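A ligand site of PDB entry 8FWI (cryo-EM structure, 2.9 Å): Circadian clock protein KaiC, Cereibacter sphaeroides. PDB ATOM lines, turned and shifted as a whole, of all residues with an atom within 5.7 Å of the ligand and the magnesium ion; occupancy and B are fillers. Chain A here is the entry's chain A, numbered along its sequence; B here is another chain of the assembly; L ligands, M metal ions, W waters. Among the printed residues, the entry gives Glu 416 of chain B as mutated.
Within 4 Å of the magnesium ion: Ser 281.
The side-chain amino group of Lys 280 is in hydrogen-bond range of the backbone carbonyl oxygen of Gly 274 (3.4 Å).
OD2 of Asp 364 lies close to OG of Ser 281 (2.8 Å).
OE2 of Glu 305 lies within salt-bridge range of NE of Arg 443 of chain B, 2.7 Å away.
The guanidinium group (NH1) of Arg 435 sits at hydrogen-bond distance from the backbone carbonyl oxygen (O) of Ala 278.
The backbone carbonyl oxygen (O) of Gly 277 sits at hydrogen-bond distance from the guanidinium group (NH1) of Arg 435, at 2.5 Å.
The backbone carbonyl oxygen of Asn 313 sits at hydrogen-bond distance from the side-chain hydroxyl of Ser 316 (3.0 Å).
The side-chain amino group of Lys 441 of chain B sits close to the backbone carbonyl oxygen of Met 418 of chain B.
Water W1 lies within hydrogen-bond range of O7 of the ligand (2.9 Å) and OE2 of Glu 305 (3.0 Å).
NZ of Lys 441 of chain B lies within salt-bridge range of O1 of the ligand.
N3 of the ligand sits at hydrogen-bond distance from O of Ser 316, at 3.2 Å.
N of Gly 279 lies within hydrogen-bond range of O9 of the ligand.
The side-chain amino group (NZ) of Lys 280 is in salt-bridge range of an oxygen (O4) of the ligand, at 2.6 Å.
O8 of the ligand lies within hydrogen-bond range of OG of Ser 282.
An oxygen (O1) of the ligand is in salt-bridge range of the guanidinium group (NH1) of Arg 443 of chain B, 2.6 Å away.
A nitrogen (N2) of the ligand sits at hydrogen-bond distance from the side-chain hydroxyl (OG) of Ser 316 (3.1 Å).
O6 of the ligand is in hydrogen-bond range of N of Gly 277, 3.4 Å away.
The guanidinium group (NH2) of Arg 435 lies within hydrogen-bond range of an oxygen (O13) of the ligand, 3.2 Å away.
An oxygen (O8) of the ligand is in hydrogen-bond range of the backbone NH of Ser 282, at 3.2 Å.
A ring nitrogen (NE2) of His 447 of chain B sits at hydrogen-bond distance from an oxygen (O13) of the ligand, at 3.0 Å.
The backbone NH (N) of Ser 281 lies within hydrogen-bond range of an oxygen (O8) of the ligand (3.4 Å).
Water W1 is bound to the magnesium ion, at 1.9 Å.
The magnesium ion is bound by water W2, 1.9 Å away.
O3 of the ligand is bound to the magnesium ion, at 2.0 Å.
The magnesium ion is bound by an oxygen (O5) of the ligand (2.0 Å).
OG of Ser 281 binds the magnesium ion, at 2.1 Å.
The magnesium ion has five donor atoms within binding distance.
The side-chain sulfur (SD) of Met 456 sits close to an oxygen (O11) of the ligand, at 2.8 Å.
The backbone carbonyl oxygen (O) of Met 445 of chain B sits close to a nitrogen (N2) of the ligand (3.2 Å).
Residues that only touch the ligand: Val 275 (3.8 Å), Ala 276 (3.8 Å), Ala 278 (3.8 Å), Leu 317 (3.7 Å), Asp 458 (3.8 Å), Glu 416 of chain B (3.7 Å), Ala 442 of chain B (3.8 Å) and Ala 446 of chain B (3.5 Å).
20 residues have an atom within 4 Å of the ligand: Val 275, Ala 276, Gly 277, Ala 278, Gly 279, Lys 280, Ser 281, Ser 282, Ser 316, Leu 317, Arg 435, Met 456, Asp 458, Glu 416 of chain B, Lys 441 of chain B, Ala 442 of chain B, Arg 443 of chain B, Met 445 of chain B, Ala 446 of chain B and His 447 of chain B.
Along chain A the residues within 4 Å of the ligand span positions 275 to 458.
The nearest printed residue that does not touch the ligand is Ser 457 (4.03 Å).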
ATOM      1  N   GLY A 274     -20.616 -18.743   2.643  1.00  0.00           N
ATOM      2  CA  GLY A 274     -19.186 -18.608   2.849  1.00  0.00           C
ATOM      3  C   GLY A 274     -18.802 -17.162   3.064  1.00  0.00           C
ATOM      4  O   GLY A 274     -19.615 -16.243   2.947  1.00  0.00           O
ATOM      5  N   VAL A 275     -17.519 -16.992   3.390  1.00  0.00           N
ATOM      6  CA  VAL A 275     -16.918 -15.679   3.580  1.00  0.00           C
ATOM      7  C   VAL A 275     -16.549 -15.089   2.226  1.00  0.00           C
ATOM      8  O   VAL A 275     -16.653 -15.767   1.191  1.00  0.00           O
ATOM      9  CB  VAL A 275     -15.675 -15.743   4.494  1.00  0.00           C
ATOM     10  CG1 VAL A 275     -16.044 -16.333   5.848  1.00  0.00           C
ATOM     11  CG2 VAL A 275     -14.571 -16.545   3.822  1.00  0.00           C
ATOM     12  N   ALA A 276     -16.123 -13.832   2.217  1.00  0.00           N
ATOM     13  CA  ALA A 276     -15.818 -13.128   0.982  1.00  0.00           C
ATOM     14  C   ALA A 276     -14.541 -13.686   0.373  1.00  0.00           C
ATOM     15  O   ALA A 276     -13.550 -13.909   1.073  1.00  0.00           O
ATOM     16  CB  ALA A 276     -15.656 -11.630   1.252  1.00  0.00           C
ATOM     17  N   GLY A 277     -14.575 -13.916  -0.939  1.00  0.00           N
ATOM     18  CA  GLY A 277     -13.493 -14.593  -1.625  1.00  0.00           C
ATOM     19  C   GLY A 277     -13.602 -16.097  -1.632  1.00  0.00           C
ATOM     20  O   GLY A 277     -12.729 -16.763  -2.193  1.00  0.00           O
ATOM     21  N   ALA A 278     -14.643 -16.648  -1.009  1.00  0.00           N
ATOM     22  CA  ALA A 278     -14.732 -18.090  -0.836  1.00  0.00           C
ATOM     23  C   ALA A 278     -14.876 -18.825  -2.163  1.00  0.00           C
ATOM     24  O   ALA A 278     -14.277 -19.879  -2.364  1.00  0.00           O
ATOM     25  CB  ALA A 278     -15.902 -18.428   0.092  1.00  0.00           C
ATOM     26  N   GLY A 279     -15.674 -18.271  -3.082  1.00  0.00           N
ATOM     27  CA  GLY A 279     -15.959 -18.951  -4.336  1.00  0.00           C
ATOM     28  C   GLY A 279     -17.436 -19.142  -4.585  1.00  0.00           C
ATOM     29  O   GLY A 279     -17.833 -19.947  -5.429  1.00  0.00           O
ATOM     30  N   LYS A 280     -18.262 -18.399  -3.851  1.00  0.00           N
ATOM     31  CA  LYS A 280     -19.703 -18.559  -3.968  1.00  0.00           C
ATOM     32  C   LYS A 280     -20.200 -18.197  -5.359  1.00  0.00           C
ATOM     33  O   LYS A 280     -20.968 -18.945  -5.970  1.00  0.00           O
ATOM     34  CB  LYS A 280     -20.402 -17.688  -2.920  1.00  0.00           C
ATOM     35  CG  LYS A 280     -19.919 -17.943  -1.498  1.00  0.00           C
ATOM     36  CD  LYS A 280     -20.761 -17.220  -0.446  1.00  0.00           C
ATOM     37  CE  LYS A 280     -20.921 -15.731  -0.714  1.00  0.00           C
ATOM     38  NZ  LYS A 280     -19.791 -14.938  -0.161  1.00  0.00           N
ATOM     39  N   SER A 281     -19.763 -17.056  -5.883  1.00  0.00           N
ATOM     40  CA  SER A 281     -20.201 -16.625  -7.207  1.00  0.00           C
ATOM     41  C   SER A 281     -19.725 -17.597  -8.278  1.00  0.00           C
ATOM     42  O   SER A 281     -20.444 -17.880  -9.241  1.00  0.00           O
ATOM     43  CB  SER A 281     -19.699 -15.217  -7.490  1.00  0.00           C
ATOM     44  OG  SER A 281     -20.144 -14.303  -6.503  1.00  0.00           O
ATOM     45  N   SER A 282     -18.511 -18.134  -8.114  1.00  0.00           N
ATOM     46  CA  SER A 282     -17.978 -19.070  -9.100  1.00  0.00           C
ATOM     47  C   SER A 282     -18.844 -20.331  -9.185  1.00  0.00           C
ATOM     48  O   SER A 282     -19.116 -20.823 -10.276  1.00  0.00           O
ATOM     49  CB  SER A 282     -16.539 -19.434  -8.751  1.00  0.00           C
ATOM     50  OG  SER A 282     -15.763 -18.268  -8.536  1.00  0.00           O
ATOM     51  N   LEU A 283     -19.264 -20.866  -8.033  1.00  0.00           N
ATOM     52  CA  LEU A 283     -20.091 -22.064  -8.045  1.00  0.00           C
ATOM     53  C   LEU A 283     -21.440 -21.808  -8.695  1.00  0.00           C
ATOM     54  O   LEU A 283     -21.927 -22.623  -9.481  1.00  0.00           O
ATOM     55  CB  LEU A 283     -20.285 -22.573  -6.613  1.00  0.00           C
ATOM     56  CG  LEU A 283     -20.695 -24.033  -6.437  1.00  0.00           C
ATOM     57  CD1 LEU A 283     -19.888 -24.955  -7.324  1.00  0.00           C
ATOM     58  CD2 LEU A 283     -20.559 -24.453  -4.984  1.00  0.00           C
ATOM     59  N   GLU A 305     -22.456  -6.916  -8.623  1.00  0.00           N
ATOM     60  CA  GLU A 305     -21.482  -6.793  -9.699  1.00  0.00           C
ATOM     61  C   GLU A 305     -22.198  -6.526 -11.014  1.00  0.00           C
ATOM     62  O   GLU A 305     -23.368  -6.879 -11.182  1.00  0.00           O
ATOM     63  CB  GLU A 305     -20.635  -8.063  -9.851  1.00  0.00           C
ATOM     64  CG  GLU A 305     -19.759  -8.381  -8.665  1.00  0.00           C
ATOM     65  CD  GLU A 305     -18.922  -9.634  -8.870  1.00  0.00           C
ATOM     66  OE1 GLU A 305     -19.385 -10.583  -9.547  1.00  0.00           O
ATOM     67  OE2 GLU A 305     -17.802  -9.702  -8.340  1.00  0.00           O
ATOM     68  N   ASN A 313     -14.745 -11.531 -14.915  1.00  0.00           N
ATOM     69  CA  ASN A 313     -14.277 -12.252 -13.738  1.00  0.00           C
ATOM     70  C   ASN A 313     -14.450 -13.744 -13.904  1.00  0.00           C
ATOM     71  O   ASN A 313     -13.554 -14.528 -13.561  1.00  0.00           O
ATOM     72  CB  ASN A 313     -15.042 -11.767 -12.500  1.00  0.00           C
ATOM     73  CG  ASN A 313     -14.514 -10.447 -11.979  1.00  0.00           C
ATOM     74  OD1 ASN A 313     -13.644  -9.816 -12.572  1.00  0.00           O
ATOM     75  ND2 ASN A 313     -15.057 -10.018 -10.847  1.00  0.00           N
ATOM     76  N   MET A 314     -15.595 -14.175 -14.453  1.00  0.00           N
ATOM     77  CA  MET A 314     -15.801 -15.600 -14.670  1.00  0.00           C
ATOM     78  C   MET A 314     -14.945 -16.144 -15.806  1.00  0.00           C
ATOM     79  O   MET A 314     -14.684 -17.348 -15.837  1.00  0.00           O
ATOM     80  CB  MET A 314     -17.263 -15.899 -15.022  1.00  0.00           C
ATOM     81  CG  MET A 314     -18.424 -15.663 -14.027  1.00  0.00           C
ATOM     82  SD  MET A 314     -18.577 -16.451 -12.424  1.00  0.00           S
ATOM     83  CE  MET A 314     -17.400 -15.586 -11.449  1.00  0.00           C
ATOM     84  N   SER A 316     -11.817 -15.848 -16.293  1.00  0.00           N
ATOM     85  CA  SER A 316     -10.546 -16.367 -15.789  1.00  0.00           C
ATOM     86  C   SER A 316     -10.684 -17.772 -15.222  1.00  0.00           C
ATOM     87  O   SER A 316      -9.690 -18.504 -15.176  1.00  0.00           O
ATOM     88  CB  SER A 316      -9.995 -15.422 -14.720  1.00  0.00           C
ATOM     89  OG  SER A 316     -10.743 -15.496 -13.525  1.00  0.00           O
ATOM     90  N   LEU A 317     -11.879 -18.158 -14.788  1.00  0.00           N
ATOM     91  CA  LEU A 317     -12.128 -19.497 -14.270  1.00  0.00           C
ATOM     92  C   LEU A 317     -12.496 -20.491 -15.368  1.00  0.00           C
ATOM     93  O   LEU A 317     -12.907 -21.612 -15.070  1.00  0.00           O
ATOM     94  CB  LEU A 317     -13.236 -19.455 -13.220  1.00  0.00           C
ATOM     95  CG  LEU A 317     -12.843 -18.860 -11.861  1.00  0.00           C
ATOM     96  CD1 LEU A 317     -13.970 -19.039 -10.851  1.00  0.00           C
ATOM     97  CD2 LEU A 317     -11.578 -19.489 -11.331  1.00  0.00           C
ATOM     98  N   ASP A 364     -27.620 -13.753  -6.297  1.00  0.00           N
ATOM     99  CA  ASP A 364     -26.276 -13.610  -5.746  1.00  0.00           C
ATOM    100  C   ASP A 364     -25.990 -12.162  -5.350  1.00  0.00           C
ATOM    101  O   ASP A 364     -25.834 -11.309  -6.241  1.00  0.00           O
ATOM    102  CB  ASP A 364     -25.249 -14.106  -6.754  1.00  0.00           C
ATOM    103  CG  ASP A 364     -23.826 -14.040  -6.220  1.00  0.00           C
ATOM    104  OD1 ASP A 364     -23.661 -13.846  -4.993  1.00  0.00           O
ATOM    105  OD2 ASP A 364     -22.886 -14.171  -7.016  1.00  0.00           O
ATOM    106  N   LEU A 401     -23.597 -14.693   2.336  1.00  0.00           N
ATOM    107  CA  LEU A 401     -22.320 -14.440   2.986  1.00  0.00           C
ATOM    108  C   LEU A 401     -22.381 -14.857   4.460  1.00  0.00           C
ATOM    109  O   LEU A 401     -23.316 -14.480   5.179  1.00  0.00           O
ATOM    110  CB  LEU A 401     -21.908 -12.977   2.861  1.00  0.00           C
ATOM    111  CG  LEU A 401     -20.515 -12.836   3.487  1.00  0.00           C
ATOM    112  CD1 LEU A 401     -19.407 -12.770   2.464  1.00  0.00           C
ATOM    113  CD2 LEU A 401     -20.442 -11.553   4.277  1.00  0.00           C
ATOM    114  N   ARG A 435      -8.615 -23.348   0.545  1.00  0.00           N
ATOM    115  CA  ARG A 435     -10.040 -23.434   0.254  1.00  0.00           C
ATOM    116  C   ARG A 435     -10.562 -24.834   0.549  1.00  0.00           C
ATOM    117  O   ARG A 435      -9.867 -25.839   0.373  1.00  0.00           O
ATOM    118  CB  ARG A 435     -10.304 -23.085  -1.213  1.00  0.00           C
ATOM    119  CG  ARG A 435      -9.934 -21.649  -1.586  1.00  0.00           C
ATOM    120  CD  ARG A 435     -10.221 -21.386  -3.041  1.00  0.00           C
ATOM    121  NE  ARG A 435      -9.691 -20.105  -3.486  1.00  0.00           N
ATOM    122  CZ  ARG A 435     -10.189 -18.928  -3.121  1.00  0.00           C
ATOM    123  NH1 ARG A 435     -11.250 -18.829  -2.330  1.00  0.00           N
ATOM    124  NH2 ARG A 435      -9.618 -17.813  -3.578  1.00  0.00           N
ATOM    125  N   MET A 456      -8.999 -23.451  -7.421  1.00  0.00           N
ATOM    126  CA  MET A 456      -9.501 -22.739  -8.590  1.00  0.00           C
ATOM    127  C   MET A 456      -8.394 -22.613  -9.605  1.00  0.00           C
ATOM    128  O   MET A 456      -7.210 -22.555  -9.258  1.00  0.00           O
ATOM    129  CB  MET A 456     -10.010 -21.349  -8.239  1.00  0.00           C
ATOM    130  CG  MET A 456     -11.175 -21.332  -7.319  1.00  0.00           C
ATOM    131  SD  MET A 456     -11.803 -19.675  -7.134  1.00  0.00           S
ATOM    132  CE  MET A 456     -13.161 -20.039  -6.056  1.00  0.00           C
ATOM    133  N   SER A 457      -8.778 -22.557 -10.873  1.00  0.00           N
ATOM    134  CA  SER A 457      -7.794 -22.468 -11.944  1.00  0.00           C
ATOM    135  C   SER A 457      -8.523 -22.063 -13.215  1.00  0.00           C
ATOM    136  O   SER A 457      -9.719 -21.772 -13.212  1.00  0.00           O
ATOM    137  CB  SER A 457      -7.051 -23.795 -12.087  1.00  0.00           C
ATOM    138  OG  SER A 457      -7.963 -24.858 -12.313  1.00  0.00           O
ATOM    139  N   ASP A 458      -7.777 -22.065 -14.320  1.00  0.00           N
ATOM    140  CA  ASP A 458      -8.368 -21.837 -15.625  1.00  0.00           C
ATOM    141  C   ASP A 458      -9.329 -22.946 -16.020  1.00  0.00           C
ATOM    142  O   ASP A 458     -10.076 -22.791 -16.993  1.00  0.00           O
ATOM    143  CB  ASP A 458      -7.267 -21.704 -16.672  1.00  0.00           C
ATOM    144  CG  ASP A 458      -6.461 -20.431 -16.507  1.00  0.00           C
ATOM    145  OD1 ASP A 458      -7.014 -19.434 -16.009  1.00  0.00           O
ATOM    146  OD2 ASP A 458      -5.267 -20.437 -16.874  1.00  0.00           O
ATOM    147  N   GLU B 416     -18.364  -5.558   0.187  1.00  0.00           N
ATOM    148  CA  GLU B 416     -18.927  -6.379  -0.876  1.00  0.00           C
ATOM    149  C   GLU B 416     -18.700  -5.785  -2.260  1.00  0.00           C
ATOM    150  O   GLU B 416     -18.618  -6.537  -3.235  1.00  0.00           O
ATOM    151  CB  GLU B 416     -20.400  -6.481  -0.533  1.00  0.00           C
ATOM    152  CG  GLU B 416     -21.439  -7.468  -0.974  1.00  0.00           C
ATOM    153  CD  GLU B 416     -21.175  -8.910  -0.589  1.00  0.00           C
ATOM    154  OE1 GLU B 416     -20.719  -9.192   0.543  1.00  0.00           O
ATOM    155  OE2 GLU B 416     -21.439  -9.790  -1.427  1.00  0.00           O
ATOM    156  N   MET B 418     -16.090  -4.275  -3.424  1.00  0.00           N
ATOM    157  CA  MET B 418     -14.670  -4.078  -3.634  1.00  0.00           C
ATOM    158  C   MET B 418     -14.127  -5.194  -4.518  1.00  0.00           C
ATOM    159  O   MET B 418     -14.413  -6.374  -4.300  1.00  0.00           O
ATOM    160  CB  MET B 418     -13.935  -4.050  -2.306  1.00  0.00           C
ATOM    161  CG  MET B 418     -14.286  -2.852  -1.450  1.00  0.00           C
ATOM    162  SD  MET B 418     -14.105  -1.289  -2.318  1.00  0.00           S
ATOM    163  CE  MET B 418     -14.777  -0.168  -1.093  1.00  0.00           C
ATOM    164  N   LEU B 440      -6.906 -10.736   0.578  1.00  0.00           N
ATOM    165  CA  LEU B 440      -8.153 -11.429   0.883  1.00  0.00           C
ATOM    166  C   LEU B 440      -8.947 -11.704  -0.391  1.00  0.00           C
ATOM    167  O   LEU B 440      -9.504 -12.784  -0.556  1.00  0.00           O
ATOM    168  CB  LEU B 440      -8.980 -10.587   1.843  1.00  0.00           C
ATOM    169  CG  LEU B 440     -10.241 -11.207   2.465  1.00  0.00           C
ATOM    170  CD1 LEU B 440     -10.527 -10.523   3.779  1.00  0.00           C
ATOM    171  CD2 LEU B 440     -11.445 -11.071   1.539  1.00  0.00           C
ATOM    172  N   LYS B 441      -8.998 -10.724  -1.288  1.00  0.00           N
ATOM    173  CA  LYS B 441      -9.821 -10.816  -2.473  1.00  0.00           C
ATOM    174  C   LYS B 441      -9.119 -10.111  -3.616  1.00  0.00           C
ATOM    175  O   LYS B 441      -8.562  -9.016  -3.443  1.00  0.00           O
ATOM    176  CB  LYS B 441     -11.201 -10.178  -2.239  1.00  0.00           C
ATOM    177  CG  LYS B 441     -12.082 -10.127  -3.478  1.00  0.00           C
ATOM    178  CD  LYS B 441     -13.534  -9.989  -3.079  1.00  0.00           C
ATOM    179  CE  LYS B 441     -13.768  -8.736  -2.244  1.00  0.00           C
ATOM    180  NZ  LYS B 441     -15.207  -8.527  -1.956  1.00  0.00           N
ATOM    181  N   ALA B 442      -9.144 -10.749  -4.765  1.00  0.00           N
ATOM    182  CA  ALA B 442      -8.735 -10.093  -5.995  1.00  0.00           C
ATOM    183  C   ALA B 442      -9.489 -10.726  -7.163  1.00  0.00           C
ATOM    184  O   ALA B 442      -9.042 -11.726  -7.737  1.00  0.00           O
ATOM    185  CB  ALA B 442      -7.230 -10.205  -6.160  1.00  0.00           C
ATOM    186  N   ARG B 443     -10.621 -10.135  -7.509  1.00  0.00           N
ATOM    187  CA  ARG B 443     -11.502 -10.754  -8.494  1.00  0.00           C
ATOM    188  C   ARG B 443     -10.937 -10.610  -9.903  1.00  0.00           C
ATOM    189  O   ARG B 443     -10.390  -9.564 -10.268  1.00  0.00           O
ATOM    190  CB  ARG B 443     -12.886 -10.128  -8.412  1.00  0.00           C
ATOM    191  CG  ARG B 443     -13.551 -10.327  -7.057  1.00  0.00           C
ATOM    192  CD  ARG B 443     -15.050 -10.141  -7.127  1.00  0.00           C
ATOM    193  NE  ARG B 443     -15.421  -8.757  -7.400  1.00  0.00           N
ATOM    194  CZ  ARG B 443     -16.286  -8.044  -6.695  1.00  0.00           C
ATOM    195  NH1 ARG B 443     -16.897  -8.544  -5.644  1.00  0.00           N
ATOM    196  NH2 ARG B 443     -16.545  -6.793  -7.059  1.00  0.00           N
ATOM    197  N   GLY B 444     -11.077 -11.665 -10.691  1.00  0.00           N
ATOM    198  CA  GLY B 444     -10.675 -11.645 -12.078  1.00  0.00           C
ATOM    199  C   GLY B 444      -9.244 -12.059 -12.340  1.00  0.00           C
ATOM    200  O   GLY B 444      -8.769 -11.853 -13.458  1.00  0.00           O
ATOM    201  N   MET B 445      -8.551 -12.639 -11.366  1.00  0.00           N
ATOM    202  CA  MET B 445      -7.117 -12.818 -11.546  1.00  0.00           C
ATOM    203  C   MET B 445      -6.691 -13.963 -10.641  1.00  0.00           C
ATOM    204  O   MET B 445      -7.432 -14.389  -9.742  1.00  0.00           O
ATOM    205  CB  MET B 445      -6.386 -11.546 -11.151  1.00  0.00           C
ATOM    206  CG  MET B 445      -6.498 -11.261  -9.630  1.00  0.00           C
ATOM    207  SD  MET B 445      -5.778  -9.720  -9.024  1.00  0.00           S
ATOM    208  CE  MET B 445      -6.210  -8.631 -10.361  1.00  0.00           C
ATOM    209  N   ALA B 446      -5.493 -14.474 -10.895  1.00  0.00           N
ATOM    210  CA  ALA B 446      -4.840 -15.405  -9.992  1.00  0.00           C
ATOM    211  C   ALA B 446      -3.800 -14.671  -9.141  1.00  0.00           C
ATOM    212  O   ALA B 446      -3.041 -13.846  -9.667  1.00  0.00           O
ATOM    213  CB  ALA B 446      -4.194 -16.538 -10.785  1.00  0.00           C
ATOM    214  N   HIS B 447      -3.769 -14.976  -7.854  1.00  0.00           N
ATOM    215  CA  HIS B 447      -2.878 -14.302  -6.924  1.00  0.00           C
ATOM    216  C   HIS B 447      -2.402 -15.276  -5.848  1.00  0.00           C
ATOM    217  O   HIS B 447      -2.996 -16.337  -5.638  1.00  0.00           O
ATOM    218  CB  HIS B 447      -3.557 -13.093  -6.267  1.00  0.00           C
ATOM    219  CG  HIS B 447      -4.704 -13.451  -5.380  1.00  0.00           C
ATOM    220  ND1 HIS B 447      -4.621 -13.450  -4.003  1.00  0.00           N
ATOM    221  CD2 HIS B 447      -5.973 -13.846  -5.678  1.00  0.00           C
ATOM    222  CE1 HIS B 447      -5.781 -13.809  -3.487  1.00  0.00           C
ATOM    223  NE2 HIS B 447      -6.614 -14.056  -4.480  1.00  0.00           N
HETATM  224  P1  LIG L   1     -17.911 -11.591  -3.125  1.00  0.00           P
HETATM  225  O1  LIG L   1     -17.232 -10.600  -4.038  1.00  0.00           O
HETATM  226  O2  LIG L   1     -17.947 -11.027  -1.721  1.00  0.00           O
HETATM  227  O3  LIG L   1     -19.303 -11.861  -3.608  1.00  0.00           O
HETATM  228  P2  LIG L   1     -17.672 -14.484  -3.457  1.00  0.00           P
HETATM  229  O4  LIG L   1     -18.213 -15.123  -2.199  1.00  0.00           O
HETATM  230  O5  LIG L   1     -18.772 -14.355  -4.492  1.00  0.00           O
HETATM  231  O6  LIG L   1     -17.035 -12.989  -3.138  1.00  0.00           O
HETATM  232  P3  LIG L   1     -15.878 -15.187  -5.621  1.00  0.00           P
HETATM  233  O7  LIG L   1     -16.220 -13.792  -6.097  1.00  0.00           O
HETATM  234  O8  LIG L   1     -16.488 -16.207  -6.549  1.00  0.00           O
HETATM  235  O9  LIG L   1     -16.454 -15.398  -4.080  1.00  0.00           O
HETATM  236  O10 LIG L   1     -14.237 -15.364  -5.596  1.00  0.00           O
HETATM  237  C1  LIG L   1     -13.571 -15.612  -6.809  1.00  0.00           C
HETATM  238  C2  LIG L   1     -12.190 -16.088  -6.488  1.00  0.00           C
HETATM  239  O11 LIG L   1     -11.768 -16.845  -7.444  1.00  0.00           O
HETATM  240  C3  LIG L   1     -11.108 -14.824  -6.397  1.00  0.00           C
HETATM  241  O12 LIG L   1     -11.020 -14.347  -5.003  1.00  0.00           O
HETATM  242  C4  LIG L   1     -10.008 -15.269  -6.753  1.00  0.00           C
HETATM  243  O13 LIG L   1      -9.110 -15.409  -5.559  1.00  0.00           O
HETATM  244  C5  LIG L   1     -10.280 -16.712  -7.402  1.00  0.00           C
HETATM  245  N1  LIG L   1      -9.810 -16.805  -8.629  1.00  0.00           N
HETATM  246  C6  LIG L   1     -10.417 -16.080  -9.566  1.00  0.00           C
HETATM  247  N2  LIG L   1      -9.817 -16.325 -10.738  1.00  0.00           N
HETATM  248  C7  LIG L   1      -8.838 -17.202 -10.522  1.00  0.00           C
HETATM  249  C8  LIG L   1      -7.922 -17.786 -11.358  1.00  0.00           C
HETATM  250  N3  LIG L   1      -7.719 -17.631 -12.784  1.00  0.00           N
HETATM  251  N4  LIG L   1      -7.035 -18.652 -10.880  1.00  0.00           N
HETATM  252  C9  LIG L   1      -7.041 -18.951  -9.557  1.00  0.00           C
HETATM  253  N5  LIG L   1      -7.944 -18.383  -8.730  1.00  0.00           N
HETATM  254  C10 LIG L   1      -8.839 -17.513  -9.217  1.00  0.00           C
HETATM  255 MG    MG M   1     -19.441 -12.699  -5.390  1.00  0.00          MG
HETATM  256  O   HOH W   1     -18.575 -12.330  -7.044  1.00  0.00           O
HETATM  257  O   HOH W   2     -20.879 -13.410  -4.314  1.00  0.00           O
